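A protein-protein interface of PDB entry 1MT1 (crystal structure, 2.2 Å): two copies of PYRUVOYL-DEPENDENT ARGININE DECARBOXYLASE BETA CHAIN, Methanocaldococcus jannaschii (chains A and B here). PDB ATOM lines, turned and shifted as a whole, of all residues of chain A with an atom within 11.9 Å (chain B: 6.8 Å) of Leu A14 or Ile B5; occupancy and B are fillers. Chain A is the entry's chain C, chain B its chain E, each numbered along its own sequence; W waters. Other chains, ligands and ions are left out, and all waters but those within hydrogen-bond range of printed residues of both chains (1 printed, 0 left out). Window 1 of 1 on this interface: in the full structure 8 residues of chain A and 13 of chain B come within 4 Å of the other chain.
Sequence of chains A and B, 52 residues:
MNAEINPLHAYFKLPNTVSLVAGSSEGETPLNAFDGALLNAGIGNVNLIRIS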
ATOM      1  N   PRO A   7      17.240  11.102 -17.992  1.00  0.00           N
ATOM      2  CA  PRO A   7      17.409  10.824 -19.421  1.00  0.00           C
ATOM      3  C   PRO A   7      16.095  10.706 -20.185  1.00  0.00           C
ATOM      4  O   PRO A   7      15.133  10.097 -19.714  1.00  0.00           O
ATOM      5  CB  PRO A   7      18.165   9.494 -19.423  1.00  0.00           C
ATOM      6  CG  PRO A   7      18.931   9.532 -18.134  1.00  0.00           C
ATOM      7  CD  PRO A   7      17.887  10.055 -17.183  1.00  0.00           C
ATOM      8  N   LEU A   8      16.062  11.320 -21.357  1.00  0.00           N
ATOM      9  CA  LEU A   8      14.892  11.276 -22.218  1.00  0.00           C
ATOM     10  C   LEU A   8      15.283  10.461 -23.447  1.00  0.00           C
ATOM     11  O   LEU A   8      16.467  10.236 -23.685  1.00  0.00           O
ATOM     12  CB  LEU A   8      14.478  12.696 -22.617  1.00  0.00           C
ATOM     13  CG  LEU A   8      14.128  13.601 -21.429  1.00  0.00           C
ATOM     14  CD1 LEU A   8      13.874  15.022 -21.903  1.00  0.00           C
ATOM     15  CD2 LEU A   8      12.913  13.048 -20.697  1.00  0.00           C
ATOM     16  N   HIS A   9      14.293  10.004 -24.208  1.00  0.00           N
ATOM     17  CA  HIS A   9      14.546   9.206 -25.404  1.00  0.00           C
ATOM     18  C   HIS A   9      15.387   7.974 -25.097  1.00  0.00           C
ATOM     19  O   HIS A   9      16.162   7.521 -25.938  1.00  0.00           O
ATOM     20  CB  HIS A   9      15.236  10.045 -26.487  1.00  0.00           C
ATOM     21  CG  HIS A   9      14.315  10.981 -27.205  1.00  0.00           C
ATOM     22  ND1 HIS A   9      14.754  12.142 -27.803  1.00  0.00           N
ATOM     23  CD2 HIS A   9      12.982  10.921 -27.431  1.00  0.00           C
ATOM     24  CE1 HIS A   9      13.731  12.756 -28.370  1.00  0.00           C
ATOM     25  NE2 HIS A   9      12.645  12.036 -28.158  1.00  0.00           N
ATOM     26  N   ALA A  10      15.236   7.443 -23.888  1.00  0.00           N
ATOM     27  CA  ALA A  10      15.975   6.259 -23.463  1.00  0.00           C
ATOM     28  C   ALA A  10      15.680   5.055 -24.363  1.00  0.00           C
ATOM     29  O   ALA A  10      16.587   4.307 -24.719  1.00  0.00           O
ATOM     30  CB  ALA A  10      15.646   5.923 -22.006  1.00  0.00           C
ATOM     31  N   TYR A  11      14.418   4.885 -24.748  1.00  0.00           N
ATOM     32  CA  TYR A  11      14.033   3.769 -25.610  1.00  0.00           C
ATOM     33  C   TYR A  11      14.627   3.812 -27.019  1.00  0.00           C
ATOM     34  O   TYR A  11      14.625   2.807 -27.722  1.00  0.00           O
ATOM     35  CB  TYR A  11      12.508   3.619 -25.664  1.00  0.00           C
ATOM     36  CG  TYR A  11      11.934   3.013 -24.403  1.00  0.00           C
ATOM     37  CD1 TYR A  11      11.505   1.687 -24.374  1.00  0.00           C
ATOM     38  CD2 TYR A  11      11.856   3.757 -23.226  1.00  0.00           C
ATOM     39  CE1 TYR A  11      11.015   1.116 -23.205  1.00  0.00           C
ATOM     40  CE2 TYR A  11      11.373   3.195 -22.048  1.00  0.00           C
ATOM     41  CZ  TYR A  11      10.956   1.875 -22.043  1.00  0.00           C
ATOM     42  OH  TYR A  11      10.502   1.316 -20.872  1.00  0.00           O
ATOM     43  N   PHE A  12      15.139   4.967 -27.433  1.00  0.00           N
ATOM     44  CA  PHE A  12      15.758   5.069 -28.754  1.00  0.00           C
ATOM     45  C   PHE A  12      17.256   4.772 -28.694  1.00  0.00           C
ATOM     46  O   PHE A  12      17.937   4.752 -29.715  1.00  0.00           O
ATOM     47  CB  PHE A  12      15.514   6.447 -29.365  1.00  0.00           C
ATOM     48  CG  PHE A  12      14.085   6.689 -29.751  1.00  0.00           C
ATOM     49  CD1 PHE A  12      13.486   5.930 -30.751  1.00  0.00           C
ATOM     50  CD2 PHE A  12      13.339   7.687 -29.126  1.00  0.00           C
ATOM     51  CE1 PHE A  12      12.166   6.160 -31.130  1.00  0.00           C
ATOM     52  CE2 PHE A  12      12.013   7.928 -29.497  1.00  0.00           C
ATOM     53  CZ  PHE A  12      11.427   7.165 -30.499  1.00  0.00           C
ATOM     54  N   LYS A  13      17.755   4.521 -27.490  1.00  0.00           N
ATOM     55  CA  LYS A  13      19.166   4.217 -27.289  1.00  0.00           C
ATOM     56  C   LYS A  13      19.381   2.715 -27.122  1.00  0.00           C
ATOM     57  O   LYS A  13      18.501   1.925 -27.445  1.00  0.00           O
ATOM     58  CB  LYS A  13      19.691   5.003 -26.084  1.00  0.00           C
ATOM     59  CG  LYS A  13      19.616   6.507 -26.305  1.00  0.00           C
ATOM     60  CD  LYS A  13      19.820   7.293 -25.020  1.00  0.00           C
ATOM     61  CE  LYS A  13      19.563   8.782 -25.254  1.00  0.00           C
ATOM     62  NZ  LYS A  13      19.656   9.577 -23.992  1.00  0.00           N
ATOM     63  N   LEU A  14      20.553   2.324 -26.633  1.00  0.00           N
ATOM     64  CA  LEU A  14      20.878   0.910 -26.450  1.00  0.00           C
ATOM     65  C   LEU A  14      20.234   0.345 -25.181  1.00  0.00           C
ATOM     66  O   LEU A  14      20.145   1.040 -24.169  1.00  0.00           O
ATOM     67  CB  LEU A  14      22.401   0.749 -26.377  1.00  0.00           C
ATOM     68  CG  LEU A  14      23.121  -0.220 -27.319  1.00  0.00           C
ATOM     69  CD1 LEU A  14      22.649  -0.039 -28.753  1.00  0.00           C
ATOM     70  CD2 LEU A  14      24.637  -0.009 -27.202  1.00  0.00           C
ATOM     71  N   PRO A  15      19.734  -0.910 -25.235  1.00  0.00           N
ATOM     72  CA  PRO A  15      19.102  -1.558 -24.077  1.00  0.00           C
ATOM     73  C   PRO A  15      20.094  -1.584 -22.925  1.00  0.00           C
ATOM     74  O   PRO A  15      21.287  -1.741 -23.153  1.00  0.00           O
ATOM     75  CB  PRO A  15      18.842  -2.982 -24.585  1.00  0.00           C
ATOM     76  CG  PRO A  15      18.591  -2.776 -26.046  1.00  0.00           C
ATOM     77  CD  PRO A  15      19.683  -1.793 -26.417  1.00  0.00           C
ATOM     78  N   ASN A  16      19.610  -1.422 -21.697  1.00  0.00           N
ATOM     79  CA  ASN A  16      20.497  -1.431 -20.533  1.00  0.00           C
ATOM     80  C   ASN A  16      20.183  -2.484 -19.475  1.00  0.00           C
ATOM     81  O   ASN A  16      20.663  -2.383 -18.349  1.00  0.00           O
ATOM     82  CB  ASN A  16      20.561  -0.046 -19.889  1.00  0.00           C
ATOM     83  CG  ASN A  16      19.194   0.551 -19.659  1.00  0.00           C
ATOM     84  OD1 ASN A  16      18.222  -0.164 -19.432  1.00  0.00           O
ATOM     85  ND2 ASN A  16      19.109   1.873 -19.731  1.00  0.00           N
ATOM     86  N   THR A  17      19.333  -3.452 -19.815  1.00  0.00           N
ATOM     87  CA  THR A  17      19.005  -4.546 -18.897  1.00  0.00           C
ATOM     88  C   THR A  17      18.959  -5.853 -19.682  1.00  0.00           C
ATOM     89  O   THR A  17      18.697  -5.852 -20.890  1.00  0.00           O
ATOM     90  CB  THR A  17      17.630  -4.380 -18.177  1.00  0.00           C
ATOM     91  OG1 THR A  17      16.560  -4.525 -19.120  1.00  0.00           O
ATOM     92  CG2 THR A  17      17.526  -3.029 -17.479  1.00  0.00           C
ATOM     93  N   VAL A  18      19.258  -6.951 -18.995  1.00  0.00           N
ATOM     94  CA  VAL A  18      19.234  -8.282 -19.586  1.00  0.00           C
ATOM     95  C   VAL A  18      18.485  -9.187 -18.620  1.00  0.00           C
ATOM     96  O   VAL A  18      18.713  -9.137 -17.413  1.00  0.00           O
ATOM     97  CB  VAL A  18      20.658  -8.860 -19.786  1.00  0.00           C
ATOM     98  CG1 VAL A  18      20.575 -10.300 -20.296  1.00  0.00           C
ATOM     99  CG2 VAL A  18      21.428  -8.019 -20.779  1.00  0.00           C
ATOM    100  N   ILE A  49      13.294 -10.535 -31.389  1.00  0.00           N
ATOM    101  CA  ILE A  49      14.183 -10.186 -32.493  1.00  0.00           C
ATOM    102  C   ILE A  49      15.475 -10.919 -32.157  1.00  0.00           C
ATOM    103  O   ILE A  49      16.239 -10.476 -31.292  1.00  0.00           O
ATOM    104  CB  ILE A  49      14.496  -8.677 -32.547  1.00  0.00           C
ATOM    105  CG1 ILE A  49      13.209  -7.854 -32.636  1.00  0.00           C
ATOM    106  CG2 ILE A  49      15.404  -8.381 -33.743  1.00  0.00           C
ATOM    107  CD1 ILE A  49      12.514  -7.961 -33.955  1.00  0.00           C
ATOM    108  N   ILE A  51      19.027 -11.993 -31.789  1.00  0.00           N
ATOM    109  CA  ILE A  51      20.332 -11.346 -31.923  1.00  0.00           C
ATOM    110  C   ILE A  51      21.445 -12.387 -31.861  1.00  0.00           C
ATOM    111  O   ILE A  51      21.388 -13.327 -31.065  1.00  0.00           O
ATOM    112  CB  ILE A  51      20.575 -10.241 -30.858  1.00  0.00           C
ATOM    113  CG1 ILE A  51      20.288 -10.764 -29.450  1.00  0.00           C
ATOM    114  CG2 ILE A  51      19.741  -9.015 -31.176  1.00  0.00           C
ATOM    115  CD1 ILE A  51      20.515  -9.740 -28.356  1.00  0.00           C
ATOM    116  N   ALA B   3      26.952   8.550 -30.112  1.00  0.00           N
ATOM    117  CA  ALA B   3      25.493   8.490 -29.794  1.00  0.00           C
ATOM    118  C   ALA B   3      24.925   7.097 -30.053  1.00  0.00           C
ATOM    119  O   ALA B   3      25.184   6.485 -31.094  1.00  0.00           O
ATOM    120  CB  ALA B   3      24.726   9.526 -30.612  1.00  0.00           C
ATOM    121  N   GLU B   4      24.132   6.612 -29.105  1.00  0.00           N
ATOM    122  CA  GLU B   4      23.520   5.296 -29.216  1.00  0.00           C
ATOM    123  C   GLU B   4      22.224   5.336 -30.009  1.00  0.00           C
ATOM    124  O   GLU B   4      21.533   6.355 -30.043  1.00  0.00           O
ATOM    125  CB  GLU B   4      23.238   4.723 -27.830  1.00  0.00           C
ATOM    126  CG  GLU B   4      24.475   4.494 -26.988  1.00  0.00           C
ATOM    127  CD  GLU B   4      24.166   3.820 -25.665  1.00  0.00           C
ATOM    128  OE1 GLU B   4      22.982   3.797 -25.256  1.00  0.00           O
ATOM    129  OE2 GLU B   4      25.112   3.309 -25.030  1.00  0.00           O
ATOM    130  N   ILE B   5      21.903   4.219 -30.652  1.00  0.00           N
ATOM    131  CA  ILE B   5      20.677   4.120 -31.422  1.00  0.00           C
ATOM    132  C   ILE B   5      20.193   2.686 -31.538  1.00  0.00           C
ATOM    133  O   ILE B   5      20.985   1.769 -31.751  1.00  0.00           O
ATOM    134  CB  ILE B   5      20.830   4.713 -32.852  1.00  0.00           C
ATOM    135  CG1 ILE B   5      19.513   4.573 -33.624  1.00  0.00           C
ATOM    136  CG2 ILE B   5      21.963   4.021 -33.606  1.00  0.00           C
ATOM    137  CD1 ILE B   5      19.546   5.151 -35.029  1.00  0.00           C
ATOM    138  N   ASN B   6      18.898   2.493 -31.311  1.00  0.00           N
ATOM    139  CA  ASN B   6      18.284   1.185 -31.458  1.00  0.00           C
ATOM    140  C   ASN B   6      17.479   1.304 -32.755  1.00  0.00           C
ATOM    141  O   ASN B   6      16.420   1.916 -32.772  1.00  0.00           O
ATOM    142  CB  ASN B   6      17.352   0.862 -30.281  1.00  0.00           C
ATOM    143  CG  ASN B   6      16.625  -0.462 -30.463  1.00  0.00           C
ATOM    144  OD1 ASN B   6      16.506  -0.962 -31.579  1.00  0.00           O
ATOM    145  ND2 ASN B   6      16.141  -1.039 -29.367  1.00  0.00           N
ATOM    146  N   PRO B   7      17.996   0.748 -33.863  1.00  0.00           N
ATOM    147  CA  PRO B   7      17.340   0.785 -35.179  1.00  0.00           C
ATOM    148  C   PRO B   7      15.930   0.179 -35.214  1.00  0.00           C
ATOM    149  O   PRO B   7      15.139   0.511 -36.091  1.00  0.00           O
ATOM    150  CB  PRO B   7      18.312   0.000 -36.061  1.00  0.00           C
ATOM    151  CG  PRO B   7      19.635   0.270 -35.422  1.00  0.00           C
ATOM    152  CD  PRO B   7      19.303   0.076 -33.962  1.00  0.00           C
ATOM    153  N   LEU B   8      15.623  -0.699 -34.262  1.00  0.00           N
ATOM    154  CA  LEU B   8      14.305  -1.332 -34.171  1.00  0.00           C
ATOM    155  C   LEU B   8      13.266  -0.360 -33.628  1.00  0.00           C
ATOM    156  O   LEU B   8      12.067  -0.543 -33.846  1.00  0.00           O
ATOM    157  CB  LEU B   8      14.357  -2.536 -33.234  1.00  0.00           C
ATOM    158  CG  LEU B   8      15.286  -3.671 -33.646  1.00  0.00           C
ATOM    159  CD1 LEU B   8      15.493  -4.615 -32.473  1.00  0.00           C
ATOM    160  CD2 LEU B   8      14.694  -4.392 -34.843  1.00  0.00           C
ATOM    161  N   ALA B  10      14.004   3.348 -33.595  1.00  0.00           N
ATOM    162  CA  ALA B  10      14.127   4.550 -34.413  1.00  0.00           C
ATOM    163  C   ALA B  10      13.947   4.148 -35.885  1.00  0.00           C
ATOM    164  O   ALA B  10      14.878   4.229 -36.687  1.00  0.00           O
ATOM    165  CB  ALA B  10      15.501   5.198 -34.191  1.00  0.00           C
ATOM    166  N   LYS B  13      14.900   6.559 -38.768  1.00  0.00           N
ATOM    167  CA  LYS B  13      16.299   6.858 -39.032  1.00  0.00           C
ATOM    168  C   LYS B  13      16.987   5.636 -39.638  1.00  0.00           C
ATOM    169  O   LYS B  13      17.396   4.718 -38.926  1.00  0.00           O
ATOM    170  CB  LYS B  13      17.010   7.305 -37.752  1.00  0.00           C
ATOM    171  CG  LYS B  13      18.345   7.993 -38.012  1.00  0.00           C
ATOM    172  CD  LYS B  13      18.855   8.705 -36.761  1.00  0.00           C
ATOM    173  CE  LYS B  13      20.157   9.457 -37.029  1.00  0.00           C
ATOM    174  NZ  LYS B  13      21.314   8.537 -37.252  1.00  0.00           N
ATOM    175  N   LEU B  14      17.084   5.634 -40.964  1.00  0.00           N
ATOM    176  CA  LEU B  14      17.695   4.542 -41.710  1.00  0.00           C
ATOM    177  C   LEU B  14      19.214   4.616 -41.770  1.00  0.00           C
ATOM    178  O   LEU B  14      19.799   5.704 -41.764  1.00  0.00           O
ATOM    179  CB  LEU B  14      17.160   4.521 -43.148  1.00  0.00           C
ATOM    180  CG  LEU B  14      15.841   3.821 -43.489  1.00  0.00           C
ATOM    181  CD1 LEU B  14      14.670   4.474 -42.785  1.00  0.00           C
ATOM    182  CD2 LEU B  14      15.636   3.868 -45.000  1.00  0.00           C
ATOM    183  N   ASN B  47      25.817  -6.725 -31.233  1.00  0.00           N
ATOM    184  CA  ASN B  47      24.643  -7.560 -31.410  1.00  0.00           C
ATOM    185  C   ASN B  47      24.170  -7.473 -32.857  1.00  0.00           C
ATOM    186  O   ASN B  47      23.663  -6.437 -33.295  1.00  0.00           O
ATOM    187  CB  ASN B  47      23.535  -7.101 -30.467  1.00  0.00           C
ATOM    188  CG  ASN B  47      23.776  -7.538 -29.040  1.00  0.00           C
ATOM    189  OD1 ASN B  47      23.900  -8.734 -28.766  1.00  0.00           O
ATOM    190  ND2 ASN B  47      23.839  -6.578 -28.122  1.00  0.00           N
HETATM  191  O   HOH W   1      21.711   2.930 -22.755  1.00  0.00           O
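Water W1 lies within hydrogen-bond range of the backbone carbonyl oxygen (O) of Leu A14 (2.8 Å) and the side-chain carboxylate (OE1) of Glu B4 (2.9 Å).
Of the printed residues of chain B, Phe A12 touches Glu B4, Ile B5, Asn B6 and Ala B10.
Printed residues of chain B within 4 Å of Lys A13: Glu B4 (3.6 Å) and Asn B6 (3.2 Å).
Leu A14 touches just these residues of chain B: Glu B4 and Ile B5.
Of the printed residues of chain B, Ile A49 touches Leu B8 (3.97 Å).
No residue of chain A comes within 4 Å of Ala B3.
Of chain A, only Phe A12, Lys A13 and Leu A14 come within 4 Å of Glu B4.
Of chain A, only Phe A12 and Leu A14 come within 4 Å of Ile B5.
Of chain A, only Phe A12 and Lys A13 come within 4 Å of Asn B6.
No residue of chain A comes within 4 Å of Pro B7.
Ala B10 touches just one residue of chain A: Phe A12 (3.9 Å).
The nearest printed residue of chain B that does not touch Phe A12 is Pro B7 (5.8 Å).
5 positions are printed for both chains.
O of Leu A8 is in hydrogen-bond range of NZ of Lys A13 (3.3 Å).
OD1 of Asn B6 lies within hydrogen-bond range of N of Leu B8.
Of the 10 printed residues of chain B, 6 touch a printed residue of chain A.
Of the 14 printed residues of chain A, 5 touch a printed residue of chain B.
Among the printed residues, no Asp or Glu carboxylate lies within 4 Å of a Lys or Arg side-chain nitrogen of the other chain.
The backbone carbonyl oxygen (O) of Phe A12 sits at hydrogen-bond distance from the backbone NH (N) of Asn B6 (2.9 Å).
N of Leu A14 lies within hydrogen-bond range of OE1 of Glu B4.
Among the printed residues, pairs that only touch across the chains: Phe A12 with Glu B4, Phe A12 with Ile B5, Phe A12 with Ala B10, Lys A13 with Glu B4, Lys A13 with Asn B6, Leu A14 with Ile B5, Ile A49 with Leu B8 and Ile A51 with Asn B47.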
